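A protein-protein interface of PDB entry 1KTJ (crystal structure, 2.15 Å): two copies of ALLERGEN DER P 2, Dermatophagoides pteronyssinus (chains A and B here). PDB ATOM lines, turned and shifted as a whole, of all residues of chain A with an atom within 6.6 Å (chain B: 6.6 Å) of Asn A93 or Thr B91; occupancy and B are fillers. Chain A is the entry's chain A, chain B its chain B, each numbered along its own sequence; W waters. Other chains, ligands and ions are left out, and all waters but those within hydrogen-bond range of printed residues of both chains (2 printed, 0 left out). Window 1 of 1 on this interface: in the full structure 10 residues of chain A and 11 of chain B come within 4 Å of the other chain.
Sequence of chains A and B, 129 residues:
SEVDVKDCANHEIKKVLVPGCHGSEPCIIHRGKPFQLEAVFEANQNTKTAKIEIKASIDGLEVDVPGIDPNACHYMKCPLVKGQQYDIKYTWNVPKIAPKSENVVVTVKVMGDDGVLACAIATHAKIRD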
ATOM      1  N   GLY A  32     -23.508   6.273 -16.790  1.00  0.00           N
ATOM      2  CA  GLY A  32     -22.498   7.216 -16.354  1.00  0.00           C
ATOM      3  C   GLY A  32     -21.440   7.567 -17.387  1.00  0.00           C
ATOM      4  O   GLY A  32     -20.535   8.338 -17.076  1.00  0.00           O
ATOM      5  N   LYS A  33     -21.517   7.077 -18.606  1.00  0.00           N
ATOM      6  CA  LYS A  33     -20.551   7.293 -19.661  1.00  0.00           C
ATOM      7  C   LYS A  33     -21.217   7.933 -20.881  1.00  0.00           C
ATOM      8  O   LYS A  33     -22.429   7.846 -21.058  1.00  0.00           O
ATOM      9  CB  LYS A  33     -19.880   5.969 -20.073  1.00  0.00           C
ATOM     10  CG  LYS A  33     -18.903   5.489 -19.002  1.00  0.00           C
ATOM     11  CD  LYS A  33     -18.197   4.205 -19.395  1.00  0.00           C
ATOM     12  CE  LYS A  33     -17.142   3.820 -18.360  1.00  0.00           C
ATOM     13  NZ  LYS A  33     -16.362   2.628 -18.823  1.00  0.00           N
ATOM     14  N   PRO A  34     -20.439   8.688 -21.646  1.00  0.00           N
ATOM     15  CA  PRO A  34     -20.914   9.281 -22.883  1.00  0.00           C
ATOM     16  C   PRO A  34     -21.273   8.231 -23.917  1.00  0.00           C
ATOM     17  O   PRO A  34     -20.751   7.119 -23.934  1.00  0.00           O
ATOM     18  CB  PRO A  34     -19.766  10.177 -23.344  1.00  0.00           C
ATOM     19  CG  PRO A  34     -18.548   9.715 -22.626  1.00  0.00           C
ATOM     20  CD  PRO A  34     -18.999   8.936 -21.423  1.00  0.00           C
ATOM     21  N   PHE A  35     -22.289   8.511 -24.715  1.00  0.00           N
ATOM     22  CA  PHE A  35     -22.767   7.644 -25.772  1.00  0.00           C
ATOM     23  C   PHE A  35     -22.782   8.453 -27.073  1.00  0.00           C
ATOM     24  O   PHE A  35     -23.592   9.374 -27.184  1.00  0.00           O
ATOM     25  CB  PHE A  35     -24.160   7.096 -25.429  1.00  0.00           C
ATOM     26  CG  PHE A  35     -24.739   6.224 -26.512  1.00  0.00           C
ATOM     27  CD1 PHE A  35     -24.265   4.946 -26.717  1.00  0.00           C
ATOM     28  CD2 PHE A  35     -25.758   6.693 -27.330  1.00  0.00           C
ATOM     29  CE1 PHE A  35     -24.780   4.138 -27.712  1.00  0.00           C
ATOM     30  CE2 PHE A  35     -26.281   5.894 -28.327  1.00  0.00           C
ATOM     31  CZ  PHE A  35     -25.789   4.620 -28.520  1.00  0.00           C
ATOM     32  N   PRO A  66     -33.619  12.305 -20.504  1.00  0.00           N
ATOM     33  CA  PRO A  66     -33.140  13.637 -20.192  1.00  0.00           C
ATOM     34  C   PRO A  66     -31.951  14.033 -21.059  1.00  0.00           C
ATOM     35  O   PRO A  66     -31.337  13.180 -21.693  1.00  0.00           O
ATOM     36  CB  PRO A  66     -32.681  13.520 -18.742  1.00  0.00           C
ATOM     37  CG  PRO A  66     -32.280  12.106 -18.582  1.00  0.00           C
ATOM     38  CD  PRO A  66     -33.074  11.287 -19.567  1.00  0.00           C
ATOM     39  N   GLY A  67     -31.599  15.298 -21.086  1.00  0.00           N
ATOM     40  CA  GLY A  67     -30.385  15.765 -21.735  1.00  0.00           C
ATOM     41  C   GLY A  67     -30.451  15.829 -23.253  1.00  0.00           C
ATOM     42  O   GLY A  67     -29.387  15.813 -23.881  1.00  0.00           O
ATOM     43  N   TYR A  90     -23.836  13.744 -32.213  1.00  0.00           N
ATOM     44  CA  TYR A  90     -24.304  14.126 -30.877  1.00  0.00           C
ATOM     45  C   TYR A  90     -23.740  13.147 -29.848  1.00  0.00           C
ATOM     46  O   TYR A  90     -23.709  11.937 -30.101  1.00  0.00           O
ATOM     47  CB  TYR A  90     -25.828  14.153 -30.842  1.00  0.00           C
ATOM     48  CG  TYR A  90     -26.496  14.898 -29.711  1.00  0.00           C
ATOM     49  CD1 TYR A  90     -26.643  16.275 -29.751  1.00  0.00           C
ATOM     50  CD2 TYR A  90     -26.996  14.238 -28.596  1.00  0.00           C
ATOM     51  CE1 TYR A  90     -27.249  16.988 -28.735  1.00  0.00           C
ATOM     52  CE2 TYR A  90     -27.611  14.926 -27.559  1.00  0.00           C
ATOM     53  CZ  TYR A  90     -27.735  16.294 -27.639  1.00  0.00           C
ATOM     54  OH  TYR A  90     -28.346  16.994 -26.618  1.00  0.00           O
ATOM     55  N   THR A  91     -23.283  13.672 -28.714  1.00  0.00           N
ATOM     56  CA  THR A  91     -22.923  12.805 -27.598  1.00  0.00           C
ATOM     57  C   THR A  91     -23.956  12.913 -26.477  1.00  0.00           C
ATOM     58  O   THR A  91     -24.177  13.983 -25.913  1.00  0.00           O
ATOM     59  CB  THR A  91     -21.513  13.108 -27.077  1.00  0.00           C
ATOM     60  OG1 THR A  91     -20.599  12.994 -28.175  1.00  0.00           O
ATOM     61  CG2 THR A  91     -21.098  12.131 -25.982  1.00  0.00           C
ATOM     62  N   TRP A  92     -24.593  11.785 -26.158  1.00  0.00           N
ATOM     63  CA  TRP A  92     -25.568  11.737 -25.080  1.00  0.00           C
ATOM     64  C   TRP A  92     -24.926  11.273 -23.783  1.00  0.00           C
ATOM     65  O   TRP A  92     -24.143  10.321 -23.796  1.00  0.00           O
ATOM     66  CB  TRP A  92     -26.740  10.830 -25.489  1.00  0.00           C
ATOM     67  CG  TRP A  92     -27.820  10.806 -24.452  1.00  0.00           C
ATOM     68  CD1 TRP A  92     -28.537  11.883 -23.999  1.00  0.00           C
ATOM     69  CD2 TRP A  92     -28.302   9.668 -23.732  1.00  0.00           C
ATOM     70  NE1 TRP A  92     -29.432  11.474 -23.038  1.00  0.00           N
ATOM     71  CE2 TRP A  92     -29.311  10.119 -22.861  1.00  0.00           C
ATOM     72  CE3 TRP A  92     -27.981   8.311 -23.744  1.00  0.00           C
ATOM     73  CZ2 TRP A  92     -30.001   9.269 -21.998  1.00  0.00           C
ATOM     74  CZ3 TRP A  92     -28.664   7.470 -22.891  1.00  0.00           C
ATOM     75  CH2 TRP A  92     -29.665   7.945 -22.032  1.00  0.00           C
ATOM     76  N   ASN A  93     -25.194  11.949 -22.674  1.00  0.00           N
ATOM     77  CA  ASN A  93     -24.652  11.504 -21.375  1.00  0.00           C
ATOM     78  C   ASN A  93     -25.572  10.471 -20.726  1.00  0.00           C
ATOM     79  O   ASN A  93     -26.708  10.805 -20.364  1.00  0.00           O
ATOM     80  CB  ASN A  93     -24.477  12.724 -20.464  1.00  0.00           C
ATOM     81  CG  ASN A  93     -23.464  13.720 -21.035  1.00  0.00           C
ATOM     82  OD1 ASN A  93     -22.257  13.528 -20.932  1.00  0.00           O
ATOM     83  ND2 ASN A  93     -23.939  14.795 -21.645  1.00  0.00           N
ATOM     84  N   VAL A  94     -25.149   9.215 -20.642  1.00  0.00           N
ATOM     85  CA  VAL A  94     -25.987   8.186 -20.010  1.00  0.00           C
ATOM     86  C   VAL A  94     -26.041   8.416 -18.506  1.00  0.00           C
ATOM     87  O   VAL A  94     -25.030   8.376 -17.815  1.00  0.00           O
ATOM     88  CB  VAL A  94     -25.458   6.765 -20.281  1.00  0.00           C
ATOM     89  CG1 VAL A  94     -26.433   5.710 -19.752  1.00  0.00           C
ATOM     90  CG2 VAL A  94     -25.235   6.543 -21.773  1.00  0.00           C
ATOM     91  N   PRO A  95     -27.235   8.676 -17.984  1.00  0.00           N
ATOM     92  CA  PRO A  95     -27.423   8.836 -16.554  1.00  0.00           C
ATOM     93  C   PRO A  95     -26.734   7.733 -15.786  1.00  0.00           C
ATOM     94  O   PRO A  95     -26.846   6.531 -16.059  1.00  0.00           O
ATOM     95  CB  PRO A  95     -28.942   8.849 -16.378  1.00  0.00           C
ATOM     96  CG  PRO A  95     -29.401   9.452 -17.683  1.00  0.00           C
ATOM     97  CD  PRO A  95     -28.521   8.788 -18.720  1.00  0.00           C
ATOM     98  N   LYS A  96     -26.072   8.118 -14.700  1.00  0.00           N
ATOM     99  CA  LYS A  96     -25.445   7.175 -13.784  1.00  0.00           C
ATOM    100  C   LYS A  96     -26.459   6.214 -13.167  1.00  0.00           C
ATOM    101  O   LYS A  96     -26.139   5.092 -12.795  1.00  0.00           O
ATOM    102  CB  LYS A  96     -24.723   7.916 -12.650  1.00  0.00           C
ATOM    103  CG  LYS A  96     -23.694   7.028 -11.963  1.00  0.00           C
ATOM    104  CD  LYS A  96     -22.638   7.826 -11.219  1.00  0.00           C
ATOM    105  CE  LYS A  96     -21.242   7.255 -11.445  1.00  0.00           C
ATOM    106  NZ  LYS A  96     -21.220   5.760 -11.414  1.00  0.00           N
ATOM    107  N   PRO B  34     -18.099  18.176 -29.410  1.00  0.00           N
ATOM    108  CA  PRO B  34     -18.295  17.877 -28.005  1.00  0.00           C
ATOM    109  C   PRO B  34     -17.306  18.623 -27.125  1.00  0.00           C
ATOM    110  O   PRO B  34     -16.142  18.808 -27.476  1.00  0.00           O
ATOM    111  CB  PRO B  34     -18.130  16.367 -27.895  1.00  0.00           C
ATOM    112  CG  PRO B  34     -17.484  15.916 -29.160  1.00  0.00           C
ATOM    113  CD  PRO B  34     -17.742  16.968 -30.204  1.00  0.00           C
ATOM    114  N   PHE B  35     -17.776  19.138 -25.999  1.00  0.00           N
ATOM    115  CA  PHE B  35     -16.918  19.751 -24.994  1.00  0.00           C
ATOM    116  C   PHE B  35     -16.976  18.947 -23.705  1.00  0.00           C
ATOM    117  O   PHE B  35     -18.017  18.946 -23.041  1.00  0.00           O
ATOM    118  CB  PHE B  35     -17.358  21.199 -24.751  1.00  0.00           C
ATOM    119  CG  PHE B  35     -16.515  21.919 -23.736  1.00  0.00           C
ATOM    120  CD1 PHE B  35     -15.195  22.225 -24.009  1.00  0.00           C
ATOM    121  CD2 PHE B  35     -17.050  22.279 -22.506  1.00  0.00           C
ATOM    122  CE1 PHE B  35     -14.415  22.879 -23.072  1.00  0.00           C
ATOM    123  CE2 PHE B  35     -16.271  22.933 -21.572  1.00  0.00           C
ATOM    124  CZ  PHE B  35     -14.957  23.236 -21.850  1.00  0.00           C
ATOM    125  N   GLN B  36     -15.915  18.230 -23.366  1.00  0.00           N
ATOM    126  CA  GLN B  36     -15.898  17.340 -22.219  1.00  0.00           C
ATOM    127  C   GLN B  36     -15.450  18.064 -20.949  1.00  0.00           C
ATOM    128  O   GLN B  36     -14.493  18.844 -20.986  1.00  0.00           O
ATOM    129  CB  GLN B  36     -14.932  16.175 -22.429  1.00  0.00           C
ATOM    130  CG  GLN B  36     -15.291  15.107 -23.431  1.00  0.00           C
ATOM    131  CD  GLN B  36     -14.299  13.951 -23.421  1.00  0.00           C
ATOM    132  OE1 GLN B  36     -13.827  13.495 -24.467  1.00  0.00           O
ATOM    133  NE2 GLN B  36     -13.968  13.458 -22.229  1.00  0.00           N
ATOM    134  N   LEU B  37     -16.099  17.770 -19.825  1.00  0.00           N
ATOM    135  CA  LEU B  37     -15.638  18.357 -18.576  1.00  0.00           C
ATOM    136  C   LEU B  37     -15.861  17.439 -17.383  1.00  0.00           C
ATOM    137  O   LEU B  37     -16.782  16.627 -17.359  1.00  0.00           O
ATOM    138  CB  LEU B  37     -16.265  19.731 -18.371  1.00  0.00           C
ATOM    139  CG  LEU B  37     -17.602  19.797 -17.643  1.00  0.00           C
ATOM    140  CD1 LEU B  37     -17.354  20.149 -16.185  1.00  0.00           C
ATOM    141  CD2 LEU B  37     -18.533  20.776 -18.333  1.00  0.00           C
ATOM    142  N   GLY B  67     -29.149  22.303 -23.999  1.00  0.00           N
ATOM    143  CA  GLY B  67     -28.542  20.975 -23.983  1.00  0.00           C
ATOM    144  C   GLY B  67     -28.030  20.597 -22.607  1.00  0.00           C
ATOM    145  O   GLY B  67     -27.137  19.759 -22.464  1.00  0.00           O
ATOM    146  N   ASP B  69     -28.850  19.322 -18.793  1.00  0.00           N
ATOM    147  CA  ASP B  69     -29.802  18.666 -17.890  1.00  0.00           C
ATOM    148  C   ASP B  69     -29.666  19.292 -16.517  1.00  0.00           C
ATOM    149  O   ASP B  69     -28.677  19.102 -15.823  1.00  0.00           O
ATOM    150  CB  ASP B  69     -29.515  17.175 -17.886  1.00  0.00           C
ATOM    151  CG  ASP B  69     -30.384  16.356 -16.954  1.00  0.00           C
ATOM    152  OD1 ASP B  69     -31.253  16.885 -16.258  1.00  0.00           O
ATOM    153  OD2 ASP B  69     -30.159  15.131 -16.928  1.00  0.00           O
ATOM    154  N   TYR B  75     -26.315  12.266 -12.751  1.00  0.00           N
ATOM    155  CA  TYR B  75     -24.927  11.939 -13.042  1.00  0.00           C
ATOM    156  C   TYR B  75     -24.122  11.682 -11.775  1.00  0.00           C
ATOM    157  O   TYR B  75     -22.887  11.652 -11.769  1.00  0.00           O
ATOM    158  CB  TYR B  75     -24.275  13.044 -13.917  1.00  0.00           C
ATOM    159  CG  TYR B  75     -25.268  13.354 -15.035  1.00  0.00           C
ATOM    160  CD1 TYR B  75     -25.419  12.438 -16.077  1.00  0.00           C
ATOM    161  CD2 TYR B  75     -26.072  14.478 -14.999  1.00  0.00           C
ATOM    162  CE1 TYR B  75     -26.334  12.671 -17.080  1.00  0.00           C
ATOM    163  CE2 TYR B  75     -26.990  14.711 -16.010  1.00  0.00           C
ATOM    164  CZ  TYR B  75     -27.113  13.807 -17.035  1.00  0.00           C
ATOM    165  OH  TYR B  75     -28.027  14.022 -18.036  1.00  0.00           O
ATOM    166  N   LYS B  89     -18.898  13.883 -14.427  1.00  0.00           N
ATOM    167  CA  LYS B  89     -18.396  13.950 -15.789  1.00  0.00           C
ATOM    168  C   LYS B  89     -19.547  14.199 -16.776  1.00  0.00           C
ATOM    169  O   LYS B  89     -20.556  13.487 -16.750  1.00  0.00           O
ATOM    170  CB  LYS B  89     -17.682  12.678 -16.231  1.00  0.00           C
ATOM    171  CG  LYS B  89     -16.564  12.189 -15.329  1.00  0.00           C
ATOM    172  CD  LYS B  89     -15.776  11.067 -16.005  1.00  0.00           C
ATOM    173  CE  LYS B  89     -14.808  10.443 -15.006  1.00  0.00           C
ATOM    174  NZ  LYS B  89     -15.555   9.949 -13.807  1.00  0.00           N
ATOM    175  N   TYR B  90     -19.348  15.144 -17.679  1.00  0.00           N
ATOM    176  CA  TYR B  90     -20.413  15.585 -18.576  1.00  0.00           C
ATOM    177  C   TYR B  90     -19.794  16.069 -19.888  1.00  0.00           C
ATOM    178  O   TYR B  90     -18.783  16.776 -19.873  1.00  0.00           O
ATOM    179  CB  TYR B  90     -21.252  16.681 -17.929  1.00  0.00           C
ATOM    180  CG  TYR B  90     -22.586  16.973 -18.574  1.00  0.00           C
ATOM    181  CD1 TYR B  90     -23.702  16.228 -18.215  1.00  0.00           C
ATOM    182  CD2 TYR B  90     -22.765  17.963 -19.527  1.00  0.00           C
ATOM    183  CE1 TYR B  90     -24.944  16.450 -18.773  1.00  0.00           C
ATOM    184  CE2 TYR B  90     -24.001  18.203 -20.099  1.00  0.00           C
ATOM    185  CZ  TYR B  90     -25.086  17.442 -19.717  1.00  0.00           C
ATOM    186  OH  TYR B  90     -26.340  17.654 -20.264  1.00  0.00           O
ATOM    187  N   THR B  91     -20.330  15.596 -20.998  1.00  0.00           N
ATOM    188  CA  THR B  91     -19.984  16.067 -22.331  1.00  0.00           C
ATOM    189  C   THR B  91     -21.113  16.940 -22.882  1.00  0.00           C
ATOM    190  O   THR B  91     -22.252  16.487 -23.039  1.00  0.00           O
ATOM    191  CB  THR B  91     -19.751  14.870 -23.277  1.00  0.00           C
ATOM    192  OG1 THR B  91     -18.624  14.124 -22.780  1.00  0.00           O
ATOM    193  CG2 THR B  91     -19.468  15.279 -24.710  1.00  0.00           C
ATOM    194  N   TRP B  92     -20.820  18.204 -23.120  1.00  0.00           N
ATOM    195  CA  TRP B  92     -21.768  19.139 -23.704  1.00  0.00           C
ATOM    196  C   TRP B  92     -21.582  19.221 -25.210  1.00  0.00           C
ATOM    197  O   TRP B  92     -20.446  19.290 -25.684  1.00  0.00           O
ATOM    198  CB  TRP B  92     -21.573  20.518 -23.072  1.00  0.00           C
ATOM    199  CG  TRP B  92     -22.542  21.565 -23.539  1.00  0.00           C
ATOM    200  CD1 TRP B  92     -23.900  21.538 -23.428  1.00  0.00           C
ATOM    201  CD2 TRP B  92     -22.223  22.801 -24.182  1.00  0.00           C
ATOM    202  NE1 TRP B  92     -24.445  22.681 -23.971  1.00  0.00           N
ATOM    203  CE2 TRP B  92     -23.433  23.473 -24.432  1.00  0.00           C
ATOM    204  CE3 TRP B  92     -21.020  23.409 -24.567  1.00  0.00           C
ATOM    205  CZ2 TRP B  92     -23.489  24.716 -25.055  1.00  0.00           C
ATOM    206  CZ3 TRP B  92     -21.079  24.648 -25.183  1.00  0.00           C
ATOM    207  CH2 TRP B  92     -22.306  25.285 -25.422  1.00  0.00           C
ATOM    208  N   ASN B  93     -22.672  19.254 -25.961  1.00  0.00           N
ATOM    209  CA  ASN B  93     -22.605  19.418 -27.406  1.00  0.00           C
ATOM    210  C   ASN B  93     -22.621  20.892 -27.798  1.00  0.00           C
ATOM    211  O   ASN B  93     -23.606  21.587 -27.534  1.00  0.00           O
ATOM    212  CB  ASN B  93     -23.759  18.639 -28.056  1.00  0.00           C
ATOM    213  CG  ASN B  93     -23.575  17.143 -27.816  1.00  0.00           C
ATOM    214  OD1 ASN B  93     -22.864  16.458 -28.552  1.00  0.00           O
ATOM    215  ND2 ASN B  93     -24.208  16.642 -26.763  1.00  0.00           N
HETATM  216  O   HOH W   1     -28.357  13.079 -20.408  1.00  0.00           O
HETATM  217  O   HOH W   2     -21.492  11.024 -16.094  1.00  0.00           O
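The backbone carbonyl oxygen of Thr A91 lies within hydrogen-bond range of the side-chain amide nitrogen of Asn B93. The backbone carbonyl oxygen (O) of Thr B91 is in hydrogen-bond range of the side-chain amide nitrogen (ND2) of Asn A93.
The side-chain carboxylate (OD2) of Asp B69 lies within hydrogen-bond range of the side-chain hydroxyl (OH) of Tyr B75, 2.6 Å away. O of Gly A67 is in hydrogen-bond range of OH of Tyr A90 (3.2 Å). The side-chain hydroxyl (OH) of Tyr B90 sits at hydrogen-bond distance from the backbone carbonyl oxygen (O) of Gly B67 (3.1 Å). The side-chain hydroxyl of Tyr B90 is in hydrogen-bond range of the backbone NH of Asp B69, at 3.4 Å. N of Leu B37 is in hydrogen-bond range of O of Tyr B90, 2.9 Å away. O of Pro A66 is in hydrogen-bond range of NE1 of Trp A92 (2.9 Å).
Among the printed residues, merely in contact across the chains: Asn A93 with Tyr B90, Pro A66 with Asp B69, Tyr A90 with Asn B93, Thr A91 with Thr B91, Asn A93 with Tyr B75 and Lys A96 with Tyr B75.
Of the printed residues of chain B, Pro A66 touches Asp B69 (3.5 Å). Asn A93 touches just these residues of chain B: Tyr B75, Tyr B90 and Thr B91. Printed residues of chain A within 4 Å of Asp B69: Pro A66. Printed residues of chain A within 4 Å of Tyr B90: Asn A93 (3.5 Å). Of chain A, only Thr A91 (3.8 Å) and Asn A93 (2.8 Å) come within 4 Å of Thr B91. The nearest printed residue of chain A that does not touch Tyr B90 is Gly A67 (4.7 Å).
Hydrophobic or aromatic side chains of chain A within 4 Å of the printed part of chain B: Pro A66 and Tyr A90. Hydrophobic or aromatic side chains of chain B that line the printed part of chain A: Tyr B75 and Tyr B90. Among the printed residues, 8 pairs touch across the chains. Among the printed residues, no Asp or Glu carboxylate lies within 4 Å of a Lys or Arg side-chain nitrogen of the other chain.
Tyr A90 touches Asn B93, and with the chains exchanged Asn A93 touches Tyr B90. Thr B91 touches its own counterpart, Thr A91. Thr A91 touches Asn B93, and with the chains exchanged Asn A93 touches Thr B91. Positions printed for both chains: 34, 35, 67, 90, 91, 92 and 93. Of the 8 pairs that touch across the chains among the printed residues, 5 have their exchanged pair printed and touching as well.
Water W1 lies within hydrogen-bond range of OH of Tyr B75 (2.6 Å), O of Asn A93 (2.8 Å), O of Pro A66 (3.2 Å) and NE1 of Trp A92 (3.3 Å). Water W2 lies within hydrogen-bond range of O of Lys B89 and O of Gly A32.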
